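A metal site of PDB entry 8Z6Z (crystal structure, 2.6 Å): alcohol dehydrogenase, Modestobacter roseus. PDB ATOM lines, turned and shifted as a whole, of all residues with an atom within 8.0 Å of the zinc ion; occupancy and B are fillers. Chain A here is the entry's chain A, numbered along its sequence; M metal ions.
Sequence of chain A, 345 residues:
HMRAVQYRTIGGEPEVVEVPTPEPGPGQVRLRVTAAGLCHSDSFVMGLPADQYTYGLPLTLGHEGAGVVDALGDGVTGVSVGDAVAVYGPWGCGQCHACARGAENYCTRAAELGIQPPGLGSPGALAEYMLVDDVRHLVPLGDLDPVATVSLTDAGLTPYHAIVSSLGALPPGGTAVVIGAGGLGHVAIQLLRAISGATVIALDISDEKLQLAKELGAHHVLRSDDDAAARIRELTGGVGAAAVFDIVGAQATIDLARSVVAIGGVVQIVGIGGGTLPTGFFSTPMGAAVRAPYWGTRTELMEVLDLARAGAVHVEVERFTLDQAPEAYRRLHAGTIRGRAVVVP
The side-chain sulfur (SG) of Cys 107 sits close to the backbone NH (N) of Ala 110 (3.6 Å).
The side-chain sulfur of Cys 96 sits close to the side-chain hydroxyl of Thr 108 (3.7 Å).
The side-chain sulfur of Cys 96 sits close to the backbone NH of Ala 98 (3.8 Å).
N of Arg 109 sits close to SG of Cys 107 (3.4 Å).
The side-chain sulfur (SG) of Cys 93 lies close to the guanidinium group (NH1) of Arg 109 (3.8 Å).
N of Gly 94 lies close to SG of Cys 99 (3.2 Å).
The backbone NH of Gln 95 lies close to the side-chain sulfur of Cys 93, 3.4 Å away.
The zinc ion is bound by the side-chain sulfur (SG) of Cys 96 (2.3 Å), the side-chain sulfur (SG) of Cys 99 (2.3 Å), the side-chain sulfur (SG) of Cys 107 (2.3 Å) and the side-chain sulfur (SG) of Cys 93 (2.3 Å).
The zinc ion has four donor atoms within binding distance.
Gly 94 touches the zinc ion (N to ZN, 3.9 Å).
Five residues have an atom within 4 Å of the zinc ion: Cys 93, Gly 94, Cys 96, Cys 99 and Cys 107.
The nearest printed residue that does not touch the zinc ion is Thr 108 (4.2 Å).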
ATOM      1  N   TRP A  91      -3.697   6.205 -26.494  1.00  0.00           N
ATOM      2  CA  TRP A  91      -2.728   5.198 -26.082  1.00  0.00           C
ATOM      3  C   TRP A  91      -2.958   3.839 -26.695  1.00  0.00           C
ATOM      4  O   TRP A  91      -4.101   3.425 -26.933  1.00  0.00           O
ATOM      5  CB  TRP A  91      -2.728   5.075 -24.551  1.00  0.00           C
ATOM      6  CG  TRP A  91      -2.289   6.312 -23.830  1.00  0.00           C
ATOM      7  CD1 TRP A  91      -1.694   7.426 -24.361  1.00  0.00           C
ATOM      8  CD2 TRP A  91      -2.389   6.551 -22.431  1.00  0.00           C
ATOM      9  NE1 TRP A  91      -1.432   8.333 -23.379  1.00  0.00           N
ATOM     10  CE2 TRP A  91      -1.859   7.821 -22.183  1.00  0.00           C
ATOM     11  CE3 TRP A  91      -2.894   5.805 -21.362  1.00  0.00           C
ATOM     12  CZ2 TRP A  91      -1.807   8.369 -20.919  1.00  0.00           C
ATOM     13  CZ3 TRP A  91      -2.853   6.345 -20.107  1.00  0.00           C
ATOM     14  CH2 TRP A  91      -2.319   7.612 -19.892  1.00  0.00           C
ATOM     15  N   GLY A  92      -1.855   3.138 -26.947  1.00  0.00           N
ATOM     16  CA  GLY A  92      -1.908   1.777 -27.443  1.00  0.00           C
ATOM     17  C   GLY A  92      -0.908   0.864 -26.756  1.00  0.00           C
ATOM     18  O   GLY A  92      -0.199   1.275 -25.840  1.00  0.00           O
ATOM     19  N   CYS A  93      -0.851  -0.369 -27.238  1.00  0.00           N
ATOM     20  CA  CYS A  93      -0.030  -1.408 -26.601  1.00  0.00           C
ATOM     21  C   CYS A  93       1.480  -1.165 -26.751  1.00  0.00           C
ATOM     22  O   CYS A  93       2.256  -1.594 -25.913  1.00  0.00           O
ATOM     23  CB  CYS A  93      -0.438  -2.788 -27.139  1.00  0.00           C
ATOM     24  SG  CYS A  93       0.154  -3.195 -28.806  1.00  0.00           S
ATOM     25  N   GLY A  94       1.881  -0.488 -27.823  1.00  0.00           N
ATOM     26  CA  GLY A  94       3.284  -0.144 -28.044  1.00  0.00           C
ATOM     27  C   GLY A  94       4.034  -1.101 -28.962  1.00  0.00           C
ATOM     28  O   GLY A  94       5.111  -0.772 -29.450  1.00  0.00           O
ATOM     29  N   GLN A  95       3.446  -2.258 -29.226  1.00  0.00           N
ATOM     30  CA  GLN A  95       4.190  -3.386 -29.804  1.00  0.00           C
ATOM     31  C   GLN A  95       3.610  -3.946 -31.103  1.00  0.00           C
ATOM     32  O   GLN A  95       4.319  -4.609 -31.835  1.00  0.00           O
ATOM     33  CB  GLN A  95       4.304  -4.540 -28.808  1.00  0.00           C
ATOM     34  CG  GLN A  95       4.370  -4.184 -27.326  1.00  0.00           C
ATOM     35  CD  GLN A  95       4.185  -5.409 -26.438  1.00  0.00           C
ATOM     36  OE1 GLN A  95       3.212  -6.161 -26.585  1.00  0.00           O
ATOM     37  NE2 GLN A  95       5.104  -5.612 -25.510  1.00  0.00           N
ATOM     38  N   CYS A  96       2.322  -3.737 -31.375  1.00  0.00           N
ATOM     39  CA  CYS A  96       1.714  -4.268 -32.589  1.00  0.00           C
ATOM     40  C   CYS A  96       2.196  -3.515 -33.829  1.00  0.00           C
ATOM     41  O   CYS A  96       2.944  -2.521 -33.739  1.00  0.00           O
ATOM     42  CB  CYS A  96       0.198  -4.202 -32.487  1.00  0.00           C
ATOM     43  SG  CYS A  96      -0.530  -2.544 -32.563  1.00  0.00           S
ATOM     44  N   HIS A  97       1.784  -3.999 -35.002  1.00  0.00           N
ATOM     45  CA  HIS A  97       2.274  -3.427 -36.262  1.00  0.00           C
ATOM     46  C   HIS A  97       1.964  -1.920 -36.346  1.00  0.00           C
ATOM     47  O   HIS A  97       2.830  -1.110 -36.718  1.00  0.00           O
ATOM     48  CB  HIS A  97       1.709  -4.168 -37.488  1.00  0.00           C
ATOM     49  CG  HIS A  97       2.300  -3.723 -38.786  1.00  0.00           C
ATOM     50  ND1 HIS A  97       1.683  -2.829 -39.623  1.00  0.00           N
ATOM     51  CD2 HIS A  97       3.476  -4.042 -39.379  1.00  0.00           C
ATOM     52  CE1 HIS A  97       2.438  -2.619 -40.692  1.00  0.00           C
ATOM     53  NE2 HIS A  97       3.534  -3.336 -40.559  1.00  0.00           N
ATOM     54  N   ALA A  98       0.740  -1.572 -35.986  1.00  0.00           N
ATOM     55  CA  ALA A  98       0.305  -0.176 -35.984  1.00  0.00           C
ATOM     56  C   ALA A  98       1.078   0.666 -34.949  1.00  0.00           C
ATOM     57  O   ALA A  98       1.667   1.704 -35.285  1.00  0.00           O
ATOM     58  CB  ALA A  98      -1.201  -0.095 -35.766  1.00  0.00           C
ATOM     59  N   CYS A  99       1.094   0.217 -33.699  1.00  0.00           N
ATOM     60  CA  CYS A  99       1.819   0.960 -32.654  1.00  0.00           C
ATOM     61  C   CYS A  99       3.281   1.233 -33.039  1.00  0.00           C
ATOM     62  O   CYS A  99       3.813   2.287 -32.701  1.00  0.00           O
ATOM     63  CB  CYS A  99       1.764   0.218 -31.316  1.00  0.00           C
ATOM     64  SG  CYS A  99       0.193   0.386 -30.418  1.00  0.00           S
ATOM     65  N   ALA A 100       3.905   0.291 -33.749  1.00  0.00           N
ATOM     66  CA  ALA A 100       5.319   0.392 -34.118  1.00  0.00           C
ATOM     67  C   ALA A 100       5.619   1.480 -35.133  1.00  0.00           C
ATOM     68  O   ALA A 100       6.745   1.991 -35.143  1.00  0.00           O
ATOM     69  CB  ALA A 100       5.846  -0.945 -34.619  1.00  0.00           C
ATOM     70  N   ALA A 103       1.404   4.776 -34.776  1.00  0.00           N
ATOM     71  CA  ALA A 103      -0.022   4.988 -34.966  1.00  0.00           C
ATOM     72  C   ALA A 103      -0.795   4.252 -33.899  1.00  0.00           C
ATOM     73  O   ALA A 103      -1.626   3.379 -34.186  1.00  0.00           O
ATOM     74  CB  ALA A 103      -0.455   4.519 -36.351  1.00  0.00           C
ATOM     75  N   GLU A 104      -0.544   4.637 -32.660  1.00  0.00           N
ATOM     76  CA  GLU A 104      -1.194   4.008 -31.524  1.00  0.00           C
ATOM     77  C   GLU A 104      -2.697   4.278 -31.549  1.00  0.00           C
ATOM     78  O   GLU A 104      -3.453   3.587 -30.894  1.00  0.00           O
ATOM     79  CB  GLU A 104      -0.565   4.463 -30.195  1.00  0.00           C
ATOM     80  CG  GLU A 104       0.951   4.237 -30.133  1.00  0.00           C
ATOM     81  CD  GLU A 104       1.511   4.022 -28.732  1.00  0.00           C
ATOM     82  OE1 GLU A 104       0.757   4.116 -27.734  1.00  0.00           O
ATOM     83  OE2 GLU A 104       2.719   3.755 -28.643  1.00  0.00           O
ATOM     84  N   ASN A 105      -3.127   5.273 -32.311  1.00  0.00           N
ATOM     85  CA  ASN A 105      -4.556   5.506 -32.506  1.00  0.00           C
ATOM     86  C   ASN A 105      -5.246   4.355 -33.196  1.00  0.00           C
ATOM     87  O   ASN A 105      -6.452   4.200 -33.061  1.00  0.00           O
ATOM     88  CB  ASN A 105      -4.819   6.812 -33.270  1.00  0.00           C
ATOM     89  CG  ASN A 105      -3.973   6.971 -34.537  1.00  0.00           C
ATOM     90  OD1 ASN A 105      -2.758   6.647 -34.555  1.00  0.00           O
ATOM     91  ND2 ASN A 105      -4.588   7.505 -35.597  1.00  0.00           N
ATOM     92  N   TYR A 106      -4.506   3.566 -33.951  1.00  0.00           N
ATOM     93  CA  TYR A 106      -5.085   2.446 -34.690  1.00  0.00           C
ATOM     94  C   TYR A 106      -4.554   1.118 -34.146  1.00  0.00           C
ATOM     95  O   TYR A 106      -4.499   0.105 -34.873  1.00  0.00           O
ATOM     96  CB  TYR A 106      -4.841   2.614 -36.201  1.00  0.00           C
ATOM     97  CG  TYR A 106      -5.526   3.834 -36.819  1.00  0.00           C
ATOM     98  CD1 TYR A 106      -6.851   4.139 -36.530  1.00  0.00           C
ATOM     99  CD2 TYR A 106      -4.839   4.679 -37.677  1.00  0.00           C
ATOM    100  CE1 TYR A 106      -7.471   5.248 -37.091  1.00  0.00           C
ATOM    101  CE2 TYR A 106      -5.450   5.799 -38.237  1.00  0.00           C
ATOM    102  CZ  TYR A 106      -6.771   6.073 -37.946  1.00  0.00           C
ATOM    103  OH  TYR A 106      -7.388   7.170 -38.499  1.00  0.00           O
ATOM    104  N   CYS A 107      -4.180   1.124 -32.877  1.00  0.00           N
ATOM    105  CA  CYS A 107      -3.690  -0.055 -32.188  1.00  0.00           C
ATOM    106  C   CYS A 107      -4.729  -1.169 -32.209  1.00  0.00           C
ATOM    107  O   CYS A 107      -5.894  -0.951 -31.890  1.00  0.00           O
ATOM    108  CB  CYS A 107      -3.323   0.274 -30.756  1.00  0.00           C
ATOM    109  SG  CYS A 107      -2.910  -1.173 -29.773  1.00  0.00           S
ATOM    110  N   THR A 108      -4.289  -2.374 -32.549  1.00  0.00           N
ATOM    111  CA  THR A 108      -5.190  -3.494 -32.769  1.00  0.00           C
ATOM    112  C   THR A 108      -5.330  -4.383 -31.537  1.00  0.00           C
ATOM    113  O   THR A 108      -5.944  -5.450 -31.619  1.00  0.00           O
ATOM    114  CB  THR A 108      -4.673  -4.351 -33.929  1.00  0.00           C
ATOM    115  OG1 THR A 108      -3.307  -4.689 -33.701  1.00  0.00           O
ATOM    116  CG2 THR A 108      -4.766  -3.581 -35.219  1.00  0.00           C
ATOM    117  N   ARG A 109      -4.775  -3.970 -30.410  1.00  0.00           N
ATOM    118  CA  ARG A 109      -4.906  -4.737 -29.165  1.00  0.00           C
ATOM    119  C   ARG A 109      -5.310  -3.892 -27.958  1.00  0.00           C
ATOM    120  O   ARG A 109      -5.251  -4.354 -26.815  1.00  0.00           O
ATOM    121  CB  ARG A 109      -3.603  -5.510 -28.900  1.00  0.00           C
ATOM    122  CG  ARG A 109      -3.277  -6.495 -30.015  1.00  0.00           C
ATOM    123  CD  ARG A 109      -2.335  -7.608 -29.598  1.00  0.00           C
ATOM    124  NE  ARG A 109      -1.091  -7.057 -29.071  1.00  0.00           N
ATOM    125  CZ  ARG A 109      -0.605  -7.269 -27.842  1.00  0.00           C
ATOM    126  NH1 ARG A 109       0.531  -6.687 -27.484  1.00  0.00           N
ATOM    127  NH2 ARG A 109      -1.246  -8.062 -26.973  1.00  0.00           N
ATOM    128  N   ALA A 110      -5.802  -2.679 -28.211  1.00  0.00           N
ATOM    129  CA  ALA A 110      -6.102  -1.732 -27.142  1.00  0.00           C
ATOM    130  C   ALA A 110      -7.398  -2.099 -26.426  1.00  0.00           C
ATOM    131  O   ALA A 110      -7.446  -2.118 -25.187  1.00  0.00           O
ATOM    132  CB  ALA A 110      -6.193  -0.318 -27.690  1.00  0.00           C
ATOM    133  N   LEU A 113      -6.990  -5.235 -24.399  1.00  0.00           N
ATOM    134  CA  LEU A 113      -6.110  -5.065 -23.227  1.00  0.00           C
ATOM    135  C   LEU A 113      -6.617  -4.009 -22.256  1.00  0.00           C
ATOM    136  O   LEU A 113      -5.940  -3.710 -21.263  1.00  0.00           O
ATOM    137  CB  LEU A 113      -4.692  -4.699 -23.676  1.00  0.00           C
ATOM    138  CG  LEU A 113      -3.845  -5.819 -24.295  1.00  0.00           C
ATOM    139  CD1 LEU A 113      -2.581  -5.245 -24.938  1.00  0.00           C
ATOM    140  CD2 LEU A 113      -3.488  -6.881 -23.260  1.00  0.00           C
ATOM    141  N   ILE A 115      -6.729  -0.820 -22.654  1.00  0.00           N
ATOM    142  CA  ILE A 115      -5.965   0.440 -22.689  1.00  0.00           C
ATOM    143  C   ILE A 115      -6.916   1.587 -23.076  1.00  0.00           C
ATOM    144  O   ILE A 115      -7.673   1.474 -24.054  1.00  0.00           O
ATOM    145  CB  ILE A 115      -4.757   0.400 -23.638  1.00  0.00           C
ATOM    146  CG1 ILE A 115      -3.768  -0.688 -23.226  1.00  0.00           C
ATOM    147  CG2 ILE A 115      -3.994   1.713 -23.588  1.00  0.00           C
ATOM    148  CD1 ILE A 115      -2.632  -0.869 -24.210  1.00  0.00           C
ATOM    149  N   ARG A 136       6.813   7.347 -23.618  1.00  0.00           N
ATOM    150  CA  ARG A 136       6.596   7.555 -25.052  1.00  0.00           C
ATOM    151  C   ARG A 136       5.307   8.309 -25.366  1.00  0.00           C
ATOM    152  O   ARG A 136       5.109   8.729 -26.509  1.00  0.00           O
ATOM    153  CB  ARG A 136       6.635   6.207 -25.806  1.00  0.00           C
ATOM    154  CG  ARG A 136       5.364   5.374 -25.738  1.00  0.00           C
ATOM    155  CD  ARG A 136       5.495   4.031 -26.437  1.00  0.00           C
ATOM    156  NE  ARG A 136       4.200   3.366 -26.392  1.00  0.00           N
ATOM    157  CZ  ARG A 136       3.757   2.634 -25.364  1.00  0.00           C
ATOM    158  NH1 ARG A 136       4.510   2.418 -24.298  1.00  0.00           N
ATOM    159  NH2 ARG A 136       2.546   2.114 -25.431  1.00  0.00           N
HETATM  160 ZN    ZN M   1      -0.740  -1.734 -30.414  1.00  0.00          ZN
